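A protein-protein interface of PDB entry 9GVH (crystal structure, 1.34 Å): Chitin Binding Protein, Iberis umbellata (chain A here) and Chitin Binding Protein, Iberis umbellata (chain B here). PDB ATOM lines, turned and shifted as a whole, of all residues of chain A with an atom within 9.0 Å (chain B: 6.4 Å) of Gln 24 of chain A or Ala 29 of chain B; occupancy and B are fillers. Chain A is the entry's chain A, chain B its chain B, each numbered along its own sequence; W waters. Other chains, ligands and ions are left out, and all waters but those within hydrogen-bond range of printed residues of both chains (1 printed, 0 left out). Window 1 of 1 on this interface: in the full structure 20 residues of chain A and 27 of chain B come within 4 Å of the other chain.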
ATOM      1  N   PHE A  14     -15.201   3.507   5.164  1.00  0.00           N
ATOM      2  CA  PHE A  14     -15.368   4.623   6.089  1.00  0.00           C
ATOM      3  C   PHE A  14     -16.615   4.442   6.945  1.00  0.00           C
ATOM      4  O   PHE A  14     -16.561   4.586   8.172  1.00  0.00           O
ATOM      5  CB  PHE A  14     -15.435   5.923   5.285  1.00  0.00           C
ATOM      6  CG  PHE A  14     -15.557   7.178   6.127  1.00  0.00           C
ATOM      7  CD1 PHE A  14     -14.525   7.567   6.965  1.00  0.00           C
ATOM      8  CD2 PHE A  14     -16.686   7.983   6.050  1.00  0.00           C
ATOM      9  CE1 PHE A  14     -14.613   8.724   7.717  1.00  0.00           C
ATOM     10  CE2 PHE A  14     -16.788   9.142   6.807  1.00  0.00           C
ATOM     11  CZ  PHE A  14     -15.742   9.517   7.634  1.00  0.00           C
ATOM     12  N   ALA A  17     -16.252   1.648   9.373  1.00  0.00           N
ATOM     13  CA  ALA A  17     -15.357   2.045  10.452  1.00  0.00           C
ATOM     14  C   ALA A  17     -15.943   3.149  11.321  1.00  0.00           C
ATOM     15  O   ALA A  17     -15.192   3.916  11.931  1.00  0.00           O
ATOM     16  CB  ALA A  17     -14.000   2.476   9.886  1.00  0.00           C
ATOM     17  N   HIS A  18     -17.272   3.261  11.354  1.00  0.00           N
ATOM     18  CA  HIS A  18     -17.971   4.235  12.191  1.00  0.00           C
ATOM     19  C   HIS A  18     -17.590   5.663  11.851  1.00  0.00           C
ATOM     20  O   HIS A  18     -17.605   6.544  12.708  1.00  0.00           O
ATOM     21  CB  HIS A  18     -17.814   3.914  13.676  1.00  0.00           C
ATOM     22  CG  HIS A  18     -18.357   2.570  14.034  1.00  0.00           C
ATOM     23  ND1 HIS A  18     -17.571   1.440  14.111  1.00  0.00           N
ATOM     24  CD2 HIS A  18     -19.625   2.162  14.273  1.00  0.00           C
ATOM     25  CE1 HIS A  18     -18.328   0.400  14.415  1.00  0.00           C
ATOM     26  NE2 HIS A  18     -19.578   0.810  14.519  1.00  0.00           N
ATOM     27  N   ARG A  19     -17.290   5.886  10.573  1.00  0.00           N
ATOM     28  CA  ARG A  19     -16.851   7.183  10.073  1.00  0.00           C
ATOM     29  C   ARG A  19     -15.666   7.720  10.862  1.00  0.00           C
ATOM     30  O   ARG A  19     -15.516   8.925  11.034  1.00  0.00           O
ATOM     31  CB  ARG A  19     -18.002   8.185   9.981  1.00  0.00           C
ATOM     32  CG  ARG A  19     -19.069   7.665   9.037  1.00  0.00           C
ATOM     33  CD  ARG A  19     -20.152   8.652   8.810  1.00  0.00           C
ATOM     34  NE  ARG A  19     -21.172   8.068   7.948  1.00  0.00           N
ATOM     35  CZ  ARG A  19     -21.905   8.770   7.100  1.00  0.00           C
ATOM     36  NH1 ARG A  19     -21.716  10.071   6.943  1.00  0.00           N
ATOM     37  NH2 ARG A  19     -22.853   8.150   6.396  1.00  0.00           N
ATOM     38  N   LEU A  20     -14.831   6.805  11.353  1.00  0.00           N
ATOM     39  CA  LEU A  20     -13.660   7.172  12.147  1.00  0.00           C
ATOM     40  C   LEU A  20     -14.049   8.117  13.281  1.00  0.00           C
ATOM     41  O   LEU A  20     -13.357   9.095  13.571  1.00  0.00           O
ATOM     42  CB  LEU A  20     -12.557   7.777  11.273  1.00  0.00           C
ATOM     43  CG  LEU A  20     -12.114   6.950  10.071  1.00  0.00           C
ATOM     44  CD1 LEU A  20     -11.083   7.714   9.282  1.00  0.00           C
ATOM     45  CD2 LEU A  20     -11.564   5.590  10.513  1.00  0.00           C
ATOM     46  N   SER A  21     -15.176   7.819  13.933  1.00  0.00           N
ATOM     47  CA  SER A  21     -15.733   8.747  14.914  1.00  0.00           C
ATOM     48  C   SER A  21     -14.770   9.043  16.062  1.00  0.00           C
ATOM     49  O   SER A  21     -14.753  10.173  16.562  1.00  0.00           O
ATOM     50  CB  SER A  21     -17.061   8.218  15.443  1.00  0.00           C
ATOM     51  OG  SER A  21     -16.873   6.988  16.061  1.00  0.00           O
ATOM     52  N   ALA A  22     -13.952   8.071  16.480  1.00  0.00           N
ATOM     53  CA  ALA A  22     -12.978   8.345  17.532  1.00  0.00           C
ATOM     54  C   ALA A  22     -11.863   9.240  17.011  1.00  0.00           C
ATOM     55  O   ALA A  22     -11.365  10.111  17.738  1.00  0.00           O
ATOM     56  CB  ALA A  22     -12.416   7.042  18.108  1.00  0.00           C
ATOM     57  N   CYS A  23     -11.460   9.047  15.750  1.00  0.00           N
ATOM     58  CA  CYS A  23     -10.512   9.967  15.131  1.00  0.00           C
ATOM     59  C   CYS A  23     -11.093  11.372  15.042  1.00  0.00           C
ATOM     60  O   CYS A  23     -10.382  12.359  15.270  1.00  0.00           O
ATOM     61  CB  CYS A  23     -10.115   9.479  13.742  1.00  0.00           C
ATOM     62  SG  CYS A  23      -9.397   7.845  13.711  1.00  0.00           S
ATOM     63  N   GLN A  24     -12.390  11.488  14.702  1.00  0.00           N
ATOM     64  CA  GLN A  24     -13.015  12.807  14.660  1.00  0.00           C
ATOM     65  C   GLN A  24     -12.951  13.493  16.017  1.00  0.00           C
ATOM     66  O   GLN A  24     -12.615  14.677  16.095  1.00  0.00           O
ATOM     67  CB  GLN A  24     -14.457  12.701  14.164  1.00  0.00           C
ATOM     68  CG  GLN A  24     -14.543  12.281  12.697  1.00  0.00           C
ATOM     69  CD  GLN A  24     -15.916  12.547  12.092  1.00  0.00           C
ATOM     70  OE1 GLN A  24     -16.543  13.572  12.363  1.00  0.00           O
ATOM     71  NE2 GLN A  24     -16.375  11.641  11.251  1.00  0.00           N
ATOM     72  N   ILE A  25     -13.249  12.764  17.102  1.00  0.00           N
ATOM     73  CA  ILE A  25     -13.178  13.376  18.425  1.00  0.00           C
ATOM     74  C   ILE A  25     -11.748  13.792  18.738  1.00  0.00           C
ATOM     75  O   ILE A  25     -11.508  14.851  19.325  1.00  0.00           O
ATOM     76  CB  ILE A  25     -13.749  12.439  19.509  1.00  0.00           C
ATOM     77  CG1 ILE A  25     -15.212  12.116  19.277  1.00  0.00           C
ATOM     78  CG2 ILE A  25     -13.748  13.139  20.849  1.00  0.00           C
ATOM     79  CD1 ILE A  25     -15.855  11.401  20.468  1.00  0.00           C
ATOM     80  N   TRP A  26     -10.775  12.959  18.352  1.00  0.00           N
ATOM     81  CA  TRP A  26      -9.367  13.258  18.605  1.00  0.00           C
ATOM     82  C   TRP A  26      -8.923  14.494  17.824  1.00  0.00           C
ATOM     83  O   TRP A  26      -8.264  15.393  18.368  1.00  0.00           O
ATOM     84  CB  TRP A  26      -8.504  12.042  18.243  1.00  0.00           C
ATOM     85  CG  TRP A  26      -7.049  12.301  18.470  1.00  0.00           C
ATOM     86  CD1 TRP A  26      -6.117  12.635  17.530  1.00  0.00           C
ATOM     87  CD2 TRP A  26      -6.371  12.324  19.733  1.00  0.00           C
ATOM     88  NE1 TRP A  26      -4.895  12.838  18.124  1.00  0.00           N
ATOM     89  CE2 TRP A  26      -5.023  12.645  19.474  1.00  0.00           C
ATOM     90  CE3 TRP A  26      -6.762  12.069  21.054  1.00  0.00           C
ATOM     91  CZ2 TRP A  26      -4.070  12.741  20.487  1.00  0.00           C
ATOM     92  CZ3 TRP A  26      -5.817  12.176  22.060  1.00  0.00           C
ATOM     93  CH2 TRP A  26      -4.482  12.495  21.768  1.00  0.00           C
ATOM     94  N   ILE A  27      -9.284  14.547  16.541  1.00  0.00           N
ATOM     95  CA  ILE A  27      -8.996  15.701  15.695  1.00  0.00           C
ATOM     96  C   ILE A  27      -9.605  16.964  16.290  1.00  0.00           C
ATOM     97  O   ILE A  27      -8.961  18.025  16.329  1.00  0.00           O
ATOM     98  CB  ILE A  27      -9.519  15.404  14.271  1.00  0.00           C
ATOM     99  CG1 ILE A  27      -8.635  14.347  13.591  1.00  0.00           C
ATOM    100  CG2 ILE A  27      -9.670  16.668  13.447  1.00  0.00           C
ATOM    101  CD1 ILE A  27      -9.331  13.660  12.430  1.00  0.00           C
ATOM    102  N   HIS A  28     -10.853  16.874  16.757  1.00  0.00           N
ATOM    103  CA  HIS A  28     -11.502  18.021  17.382  1.00  0.00           C
ATOM    104  C   HIS A  28     -10.736  18.474  18.626  1.00  0.00           C
ATOM    105  O   HIS A  28     -10.444  19.666  18.790  1.00  0.00           O
ATOM    106  CB  HIS A  28     -12.937  17.616  17.714  1.00  0.00           C
ATOM    107  CG  HIS A  28     -13.751  18.684  18.372  1.00  0.00           C
ATOM    108  ND1 HIS A  28     -14.946  18.400  18.999  1.00  0.00           N
ATOM    109  CD2 HIS A  28     -13.577  20.021  18.475  1.00  0.00           C
ATOM    110  CE1 HIS A  28     -15.459  19.518  19.482  1.00  0.00           C
ATOM    111  NE2 HIS A  28     -14.644  20.513  19.185  1.00  0.00           N
ATOM    112  N   SER A  29     -10.383  17.531  19.501  1.00  0.00           N
ATOM    113  CA  SER A  29      -9.634  17.838  20.719  1.00  0.00           C
ATOM    114  C   SER A  29      -8.321  18.534  20.397  1.00  0.00           C
ATOM    115  O   SER A  29      -7.966  19.538  21.029  1.00  0.00           O
ATOM    116  CB  SER A  29      -9.382  16.541  21.496  1.00  0.00           C
ATOM    117  OG  SER A  29      -8.517  16.719  22.605  1.00  0.00           O
ATOM    118  N   GLU A  30      -7.592  18.040  19.395  1.00  0.00           N
ATOM    119  CA  GLU A  30      -6.318  18.669  19.061  1.00  0.00           C
ATOM    120  C   GLU A  30      -6.517  20.045  18.446  1.00  0.00           C
ATOM    121  O   GLU A  30      -5.744  20.970  18.731  1.00  0.00           O
ATOM    122  CB  GLU A  30      -5.515  17.781  18.114  1.00  0.00           C
ATOM    123  CG  GLU A  30      -4.938  16.531  18.767  1.00  0.00           C
ATOM    124  CD  GLU A  30      -3.918  16.837  19.834  1.00  0.00           C
ATOM    125  OE1 GLU A  30      -3.289  17.920  19.769  1.00  0.00           O
ATOM    126  OE2 GLU A  30      -3.743  16.017  20.754  1.00  0.00           O
ATOM    127  N   ALA A  31      -7.540  20.201  17.600  1.00  0.00           N
ATOM    128  CA  ALA A  31      -7.775  21.480  16.937  1.00  0.00           C
ATOM    129  C   ALA A  31      -7.992  22.592  17.947  1.00  0.00           C
ATOM    130  O   ALA A  31      -7.414  23.681  17.821  1.00  0.00           O
ATOM    131  CB  ALA A  31      -8.979  21.379  16.001  1.00  0.00           C
ATOM    132  N   CYS B  10      -9.264   5.484  17.897  1.00  0.00           N
ATOM    133  CA  CYS B  10      -9.112   5.981  16.537  1.00  0.00           C
ATOM    134  C   CYS B  10      -8.267   5.031  15.694  1.00  0.00           C
ATOM    135  O   CYS B  10      -8.624   4.712  14.557  1.00  0.00           O
ATOM    136  CB  CYS B  10      -8.478   7.363  16.594  1.00  0.00           C
ATOM    137  SG  CYS B  10      -7.832   7.933  15.016  1.00  0.00           S
ATOM    138  N   GLN B  13     -10.242   1.978  14.667  1.00  0.00           N
ATOM    139  CA  GLN B  13     -11.136   2.274  13.554  1.00  0.00           C
ATOM    140  C   GLN B  13     -10.367   2.426  12.245  1.00  0.00           C
ATOM    141  O   GLN B  13     -10.804   1.913  11.201  1.00  0.00           O
ATOM    142  CB  GLN B  13     -11.939   3.529  13.872  1.00  0.00           C
ATOM    143  CG  GLN B  13     -12.890   3.358  15.052  1.00  0.00           C
ATOM    144  CD  GLN B  13     -13.658   4.620  15.378  1.00  0.00           C
ATOM    145  OE1 GLN B  13     -13.181   5.720  15.148  1.00  0.00           O
ATOM    146  NE2 GLN B  13     -14.853   4.466  15.924  1.00  0.00           N
ATOM    147  N   SER B  24      -7.692   9.648   2.206  1.00  0.00           N
ATOM    148  CA  SER B  24      -8.962  10.159   1.698  1.00  0.00           C
ATOM    149  C   SER B  24     -10.023  10.191   2.797  1.00  0.00           C
ATOM    150  O   SER B  24     -10.760  11.176   2.938  1.00  0.00           O
ATOM    151  CB  SER B  24      -9.414   9.280   0.527  1.00  0.00           C
ATOM    152  OG  SER B  24     -10.689   9.661   0.030  1.00  0.00           O
ATOM    153  N   THR B  25     -10.115   9.122   3.590  1.00  0.00           N
ATOM    154  CA  THR B  25     -11.135   9.086   4.638  1.00  0.00           C
ATOM    155  C   THR B  25     -10.794  10.015   5.793  1.00  0.00           C
ATOM    156  O   THR B  25     -11.700  10.567   6.432  1.00  0.00           O
ATOM    157  CB  THR B  25     -11.354   7.661   5.143  1.00  0.00           C
ATOM    158  OG1 THR B  25     -10.135   7.162   5.709  1.00  0.00           O
ATOM    159  CG2 THR B  25     -11.843   6.745   4.018  1.00  0.00           C
ATOM    160  N   LEU B  26      -9.507  10.219   6.073  1.00  0.00           N
ATOM    161  CA  LEU B  26      -9.141  11.185   7.106  1.00  0.00           C
ATOM    162  C   LEU B  26      -9.426  12.616   6.665  1.00  0.00           C
ATOM    163  O   LEU B  26      -9.796  13.443   7.499  1.00  0.00           O
ATOM    164  CB  LEU B  26      -7.679  11.017   7.516  1.00  0.00           C
ATOM    165  CG  LEU B  26      -7.440   9.830   8.445  1.00  0.00           C
ATOM    166  CD1 LEU B  26      -5.966   9.499   8.510  1.00  0.00           C
ATOM    167  CD2 LEU B  26      -8.005  10.085   9.856  1.00  0.00           C
ATOM    168  N   ARG B  27      -9.264  12.921   5.374  1.00  0.00           N
ATOM    169  CA  ARG B  27      -9.675  14.224   4.854  1.00  0.00           C
ATOM    170  C   ARG B  27     -11.177  14.416   5.033  1.00  0.00           C
ATOM    171  O   ARG B  27     -11.645  15.477   5.484  1.00  0.00           O
ATOM    172  CB  ARG B  27      -9.291  14.301   3.373  1.00  0.00           C
ATOM    173  CG  ARG B  27      -9.856  15.494   2.617  1.00  0.00           C
ATOM    174  CD  ARG B  27      -9.041  16.737   2.818  1.00  0.00           C
ATOM    175  NE  ARG B  27      -9.435  17.780   1.875  1.00  0.00           N
ATOM    176  CZ  ARG B  27      -8.839  18.960   1.777  1.00  0.00           C
ATOM    177  NH1 ARG B  27      -7.842  19.300   2.580  1.00  0.00           N
ATOM    178  NH2 ARG B  27      -9.261  19.825   0.859  1.00  0.00           N
ATOM    179  N   ARG B  28     -11.954  13.383   4.704  1.00  0.00           N
ATOM    180  CA  ARG B  28     -13.394  13.446   4.907  1.00  0.00           C
ATOM    181  C   ARG B  28     -13.733  13.659   6.377  1.00  0.00           C
ATOM    182  O   ARG B  28     -14.606  14.473   6.704  1.00  0.00           O
ATOM    183  CB  ARG B  28     -14.031  12.167   4.375  1.00  0.00           C
ATOM    184  CG  ARG B  28     -15.510  12.114   4.533  1.00  0.00           C
ATOM    185  CD  ARG B  28     -16.074  10.913   3.834  1.00  0.00           C
ATOM    186  NE  ARG B  28     -17.485  10.787   4.158  1.00  0.00           N
ATOM    187  CZ  ARG B  28     -18.273   9.825   3.705  1.00  0.00           C
ATOM    188  NH1 ARG B  28     -17.816   8.888   2.885  1.00  0.00           N
ATOM    189  NH2 ARG B  28     -19.547   9.799   4.087  1.00  0.00           N
ATOM    190  N   ALA B  29     -13.062  12.931   7.277  1.00  0.00           N
ATOM    191  CA  ALA B  29     -13.311  13.072   8.708  1.00  0.00           C
ATOM    192  C   ALA B  29     -12.979  14.478   9.191  1.00  0.00           C
ATOM    193  O   ALA B  29     -13.701  15.046  10.028  1.00  0.00           O
ATOM    194  CB  ALA B  29     -12.468  12.047   9.476  1.00  0.00           C
ATOM    195  N   ALA B  30     -11.869  15.040   8.703  1.00  0.00           N
ATOM    196  CA  ALA B  30     -11.483  16.392   9.088  1.00  0.00           C
ATOM    197  C   ALA B  30     -12.527  17.414   8.633  1.00  0.00           C
ATOM    198  O   ALA B  30     -12.901  18.322   9.390  1.00  0.00           O
ATOM    199  CB  ALA B  30     -10.099  16.704   8.512  1.00  0.00           C
ATOM    200  N   MET B  31     -13.006  17.287   7.394  1.00  0.00           N
ATOM    201  CA  MET B  31     -14.041  18.208   6.921  1.00  0.00           C
ATOM    202  C   MET B  31     -15.317  18.071   7.735  1.00  0.00           C
ATOM    203  O   MET B  31     -15.987  19.072   8.032  1.00  0.00           O
ATOM    204  CB  MET B  31     -14.334  17.948   5.447  1.00  0.00           C
ATOM    205  CG  MET B  31     -13.158  18.245   4.545  1.00  0.00           C
ATOM    206  SD  MET B  31     -13.586  17.978   2.829  1.00  0.00           S
ATOM    207  CE  MET B  31     -14.674  16.559   2.950  1.00  0.00           C
ATOM    208  N   ALA B  32     -15.661  16.843   8.124  1.00  0.00           N
ATOM    209  CA  ALA B  32     -16.858  16.624   8.924  1.00  0.00           C
ATOM    210  C   ALA B  32     -16.754  17.334  10.270  1.00  0.00           C
ATOM    211  O   ALA B  32     -17.678  18.046  10.678  1.00  0.00           O
ATOM    212  CB  ALA B  32     -17.104  15.126   9.088  1.00  0.00           C
ATOM    213  N   THR B  33     -15.610  17.199  10.949  1.00  0.00           N
ATOM    214  CA  THR B  33     -15.403  17.876  12.231  1.00  0.00           C
ATOM    215  C   THR B  33     -15.418  19.384  12.056  1.00  0.00           C
ATOM    216  O   THR B  33     -16.075  20.112  12.814  1.00  0.00           O
ATOM    217  CB  THR B  33     -14.054  17.458  12.842  1.00  0.00           C
ATOM    218  OG1 THR B  33     -14.109  16.077  13.227  1.00  0.00           O
ATOM    219  CG2 THR B  33     -13.722  18.322  14.078  1.00  0.00           C
ATOM    220  N   ARG B  34     -14.677  19.877  11.064  1.00  0.00           N
ATOM    221  CA  ARG B  34     -14.576  21.316  10.876  1.00  0.00           C
ATOM    222  C   ARG B  34     -15.958  21.930  10.685  1.00  0.00           C
ATOM    223  O   ARG B  34     -16.292  22.949  11.306  1.00  0.00           O
ATOM    224  CB  ARG B  34     -13.669  21.587   9.678  1.00  0.00           C
ATOM    225  CG  ARG B  34     -13.174  23.021   9.549  1.00  0.00           C
ATOM    226  CD  ARG B  34     -14.166  23.931   8.848  1.00  0.00           C
ATOM    227  NE  ARG B  34     -13.584  25.232   8.533  1.00  0.00           N
ATOM    228  CZ  ARG B  34     -12.958  25.502   7.396  1.00  0.00           C
ATOM    229  NH1 ARG B  34     -12.841  24.595   6.446  1.00  0.00           N
ATOM    230  NH2 ARG B  34     -12.433  26.712   7.211  1.00  0.00           N
ATOM    231  N   ARG B  36     -19.148  20.412  11.273  1.00  0.00           N
ATOM    232  CA  ARG B  36     -20.084  20.155  12.366  1.00  0.00           C
ATOM    233  C   ARG B  36     -19.805  21.058  13.554  1.00  0.00           C
ATOM    234  O   ARG B  36     -20.735  21.542  14.209  1.00  0.00           O
ATOM    235  CB  ARG B  36     -19.988  18.707  12.836  1.00  0.00           C
ATOM    236  CG  ARG B  36     -20.895  17.731  12.151  1.00  0.00           C
ATOM    237  CD  ARG B  36     -21.252  16.553  13.078  1.00  0.00           C
ATOM    238  NE  ARG B  36     -20.099  16.105  13.856  1.00  0.00           N
ATOM    239  CZ  ARG B  36     -19.121  15.335  13.394  1.00  0.00           C
ATOM    240  NH1 ARG B  36     -19.141  14.850  12.162  1.00  0.00           N
ATOM    241  NH2 ARG B  36     -18.085  15.064  14.186  1.00  0.00           N
ATOM    242  N   LEU B  48      -6.408  21.168  12.975  1.00  0.00           N
ATOM    243  CA  LEU B  48      -7.385  20.118  12.715  1.00  0.00           C
ATOM    244  C   LEU B  48      -6.937  19.243  11.553  1.00  0.00           C
ATOM    245  O   LEU B  48      -6.826  18.013  11.676  1.00  0.00           O
ATOM    246  CB  LEU B  48      -8.713  20.805  12.391  1.00  0.00           C
ATOM    247  CG  LEU B  48      -9.987  19.972  12.354  1.00  0.00           C
ATOM    248  CD1 LEU B  48     -11.164  20.920  12.483  1.00  0.00           C
ATOM    249  CD2 LEU B  48     -10.124  19.192  11.090  1.00  0.00           C
ATOM    250  N   ALA B  52      -5.271  15.286  11.516  1.00  0.00           N
ATOM    251  CA  ALA B  52      -5.804  14.205  10.692  1.00  0.00           C
ATOM    252  C   ALA B  52      -4.728  13.603   9.804  1.00  0.00           C
ATOM    253  O   ALA B  52      -4.606  12.376   9.719  1.00  0.00           O
ATOM    254  CB  ALA B  52      -6.997  14.699   9.862  1.00  0.00           C
ATOM    255  N   LEU B  55      -2.298  11.069  11.595  1.00  0.00           N
ATOM    256  CA  LEU B  55      -2.784   9.855  12.255  1.00  0.00           C
ATOM    257  C   LEU B  55      -2.256   8.539  11.691  1.00  0.00           C
ATOM    258  O   LEU B  55      -2.065   7.602  12.488  1.00  0.00           O
ATOM    259  CB  LEU B  55      -4.315   9.853  12.324  1.00  0.00           C
ATOM    260  CG  LEU B  55      -4.903  10.757  13.408  1.00  0.00           C
ATOM    261  CD1 LEU B  55      -6.400  10.922  13.238  1.00  0.00           C
ATOM    262  CD2 LEU B  55      -4.578  10.225  14.811  1.00  0.00           C
HETATM  263  O   HOH W   1     -19.242  12.370   6.071  1.00  0.00           O
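Of chain B, only Ala 29, Ala 32, Thr 33 and Arg 36 come within 4 Å of Gln 24 of chain A.
Of the printed residues of chain B, Trp 26 of chain A touches Leu 55.
Of the printed residues of chain A, Thr 25 of chain B touches Phe 14 (3.7 Å) and Leu 20 (3.7 Å).
Of the printed residues of chain A, Leu 26 of chain B touches Leu 20.
Ala 29 of chain B touches just one residue of chain A: Gln 24.
No residue of chain A comes within 4 Å of Ala 30 of chain B.
Arg 34 of chain B touches none of the printed residues of chain A.
Of the printed residues of chain A, Leu 55 of chain B touches Trp 26.
The nearest residue of chain B that does not touch Gln 24 of chain A is Ala 30 of chain B (5.5 Å).
The nearest printed residue of chain B that does not touch Arg 19 of chain A is Ala 29 of chain B (4.6 Å).
Water W1 lies within hydrogen-bond range of the guanidinium group of Arg 28 of chain B (3.0 Å) and the guanidinium group of Arg 19 of chain A (3.5 Å).
N of Ser 21 of chain A lies within hydrogen-bond range of OE1 of Gln 13 of chain B (3.1 Å).
The backbone NH (N) of Ala 22 of chain A is in hydrogen-bond range of the side-chain amide oxygen (OE1) of Gln 13 of chain B.
SG of Cys 23 of chain A is disulfide-bonded to SG of Cys 10 of chain B (2.0 Å).
NH2 of Arg 36 of chain B lies within hydrogen-bond range of OE1 of Gln 24 of chain A, at 2.8 Å.
O of Phe 14 of chain A is in hydrogen-bond range of N of Arg 19 of chain A (2.8 Å).
OG of Ser 21 of chain A sits close to O of His 18 of chain A.
The backbone carbonyl oxygen (O) of Arg 19 of chain A lies within hydrogen-bond range of the side-chain amide nitrogen (NE2) of Gln 24 of chain A.
The side-chain hydroxyl of Thr 33 of chain B lies within hydrogen-bond range of the backbone carbonyl oxygen of Ala 29 of chain B (3.4 Å).
Printed residues of chain B that touch a printed residue of chain A: Cys 10, Gln 13, Thr 25, Leu 26, Arg 28, Ala 29, Ala 32, Thr 33, Arg 36, Leu 48, Ala 52 and Leu 55.
Of the 16 printed residues of chain A, 13 touch a printed residue of chain B.
Hydrophobic or aromatic side chains of chain A within 4 Å of the printed part of chain B: Phe 14, Ala 17, His 18, Leu 20, Ala 22, Trp 26, Ile 27, His 28 and Ala 31.
Among the printed residues, 22 pairs touch across the chains.
Among the printed residues, no Asp or Glu carboxylate lies within 4 Å of a Lys or Arg side-chain nitrogen of the other chain.
Among the printed residues, pairs that only touch across the chains: Leu 20 of chain A with Gln 13 of chain B (3.2 Å), Phe 14 of chain A with Arg 28 of chain B (3.2 Å), Ile 27 of chain A with Leu 48 of chain B (3.5 Å), Ala 17 of chain A with Gln 13 of chain B (3.5 Å), Gln 24 of chain A with Thr 33 of chain B (3.5 Å), Ala 22 of chain A with Cys 10 of chain B (3.5 Å), Arg 19 of chain A with Arg 28 of chain B (3.6 Å), Ile 27 of chain A with Ala 52 of chain B (3.6 Å), Phe 14 of chain A with Thr 25 of chain B (3.7 Å), Ala 31 of chain A with Leu 48 of chain B (3.7 Å), Gln 24 of chain A with Ala 32 of chain B (3.7 Å), Leu 20 of chain A with Thr 25 of chain B (3.7 Å), His 18 of chain A with Gln 13 of chain B (3.8 Å), His 28 of chain A with Thr 33 of chain B (3.8 Å), Cys 23 of chain A with Gln 13 of chain B (3.8 Å), Gln 24 of chain A with Ala 29 of chain B (3.8 Å), Leu 20 of chain A with Leu 26 of chain B (3.9 Å) and Trp 26 of chain A with Leu 55 of chain B (3.9 Å).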
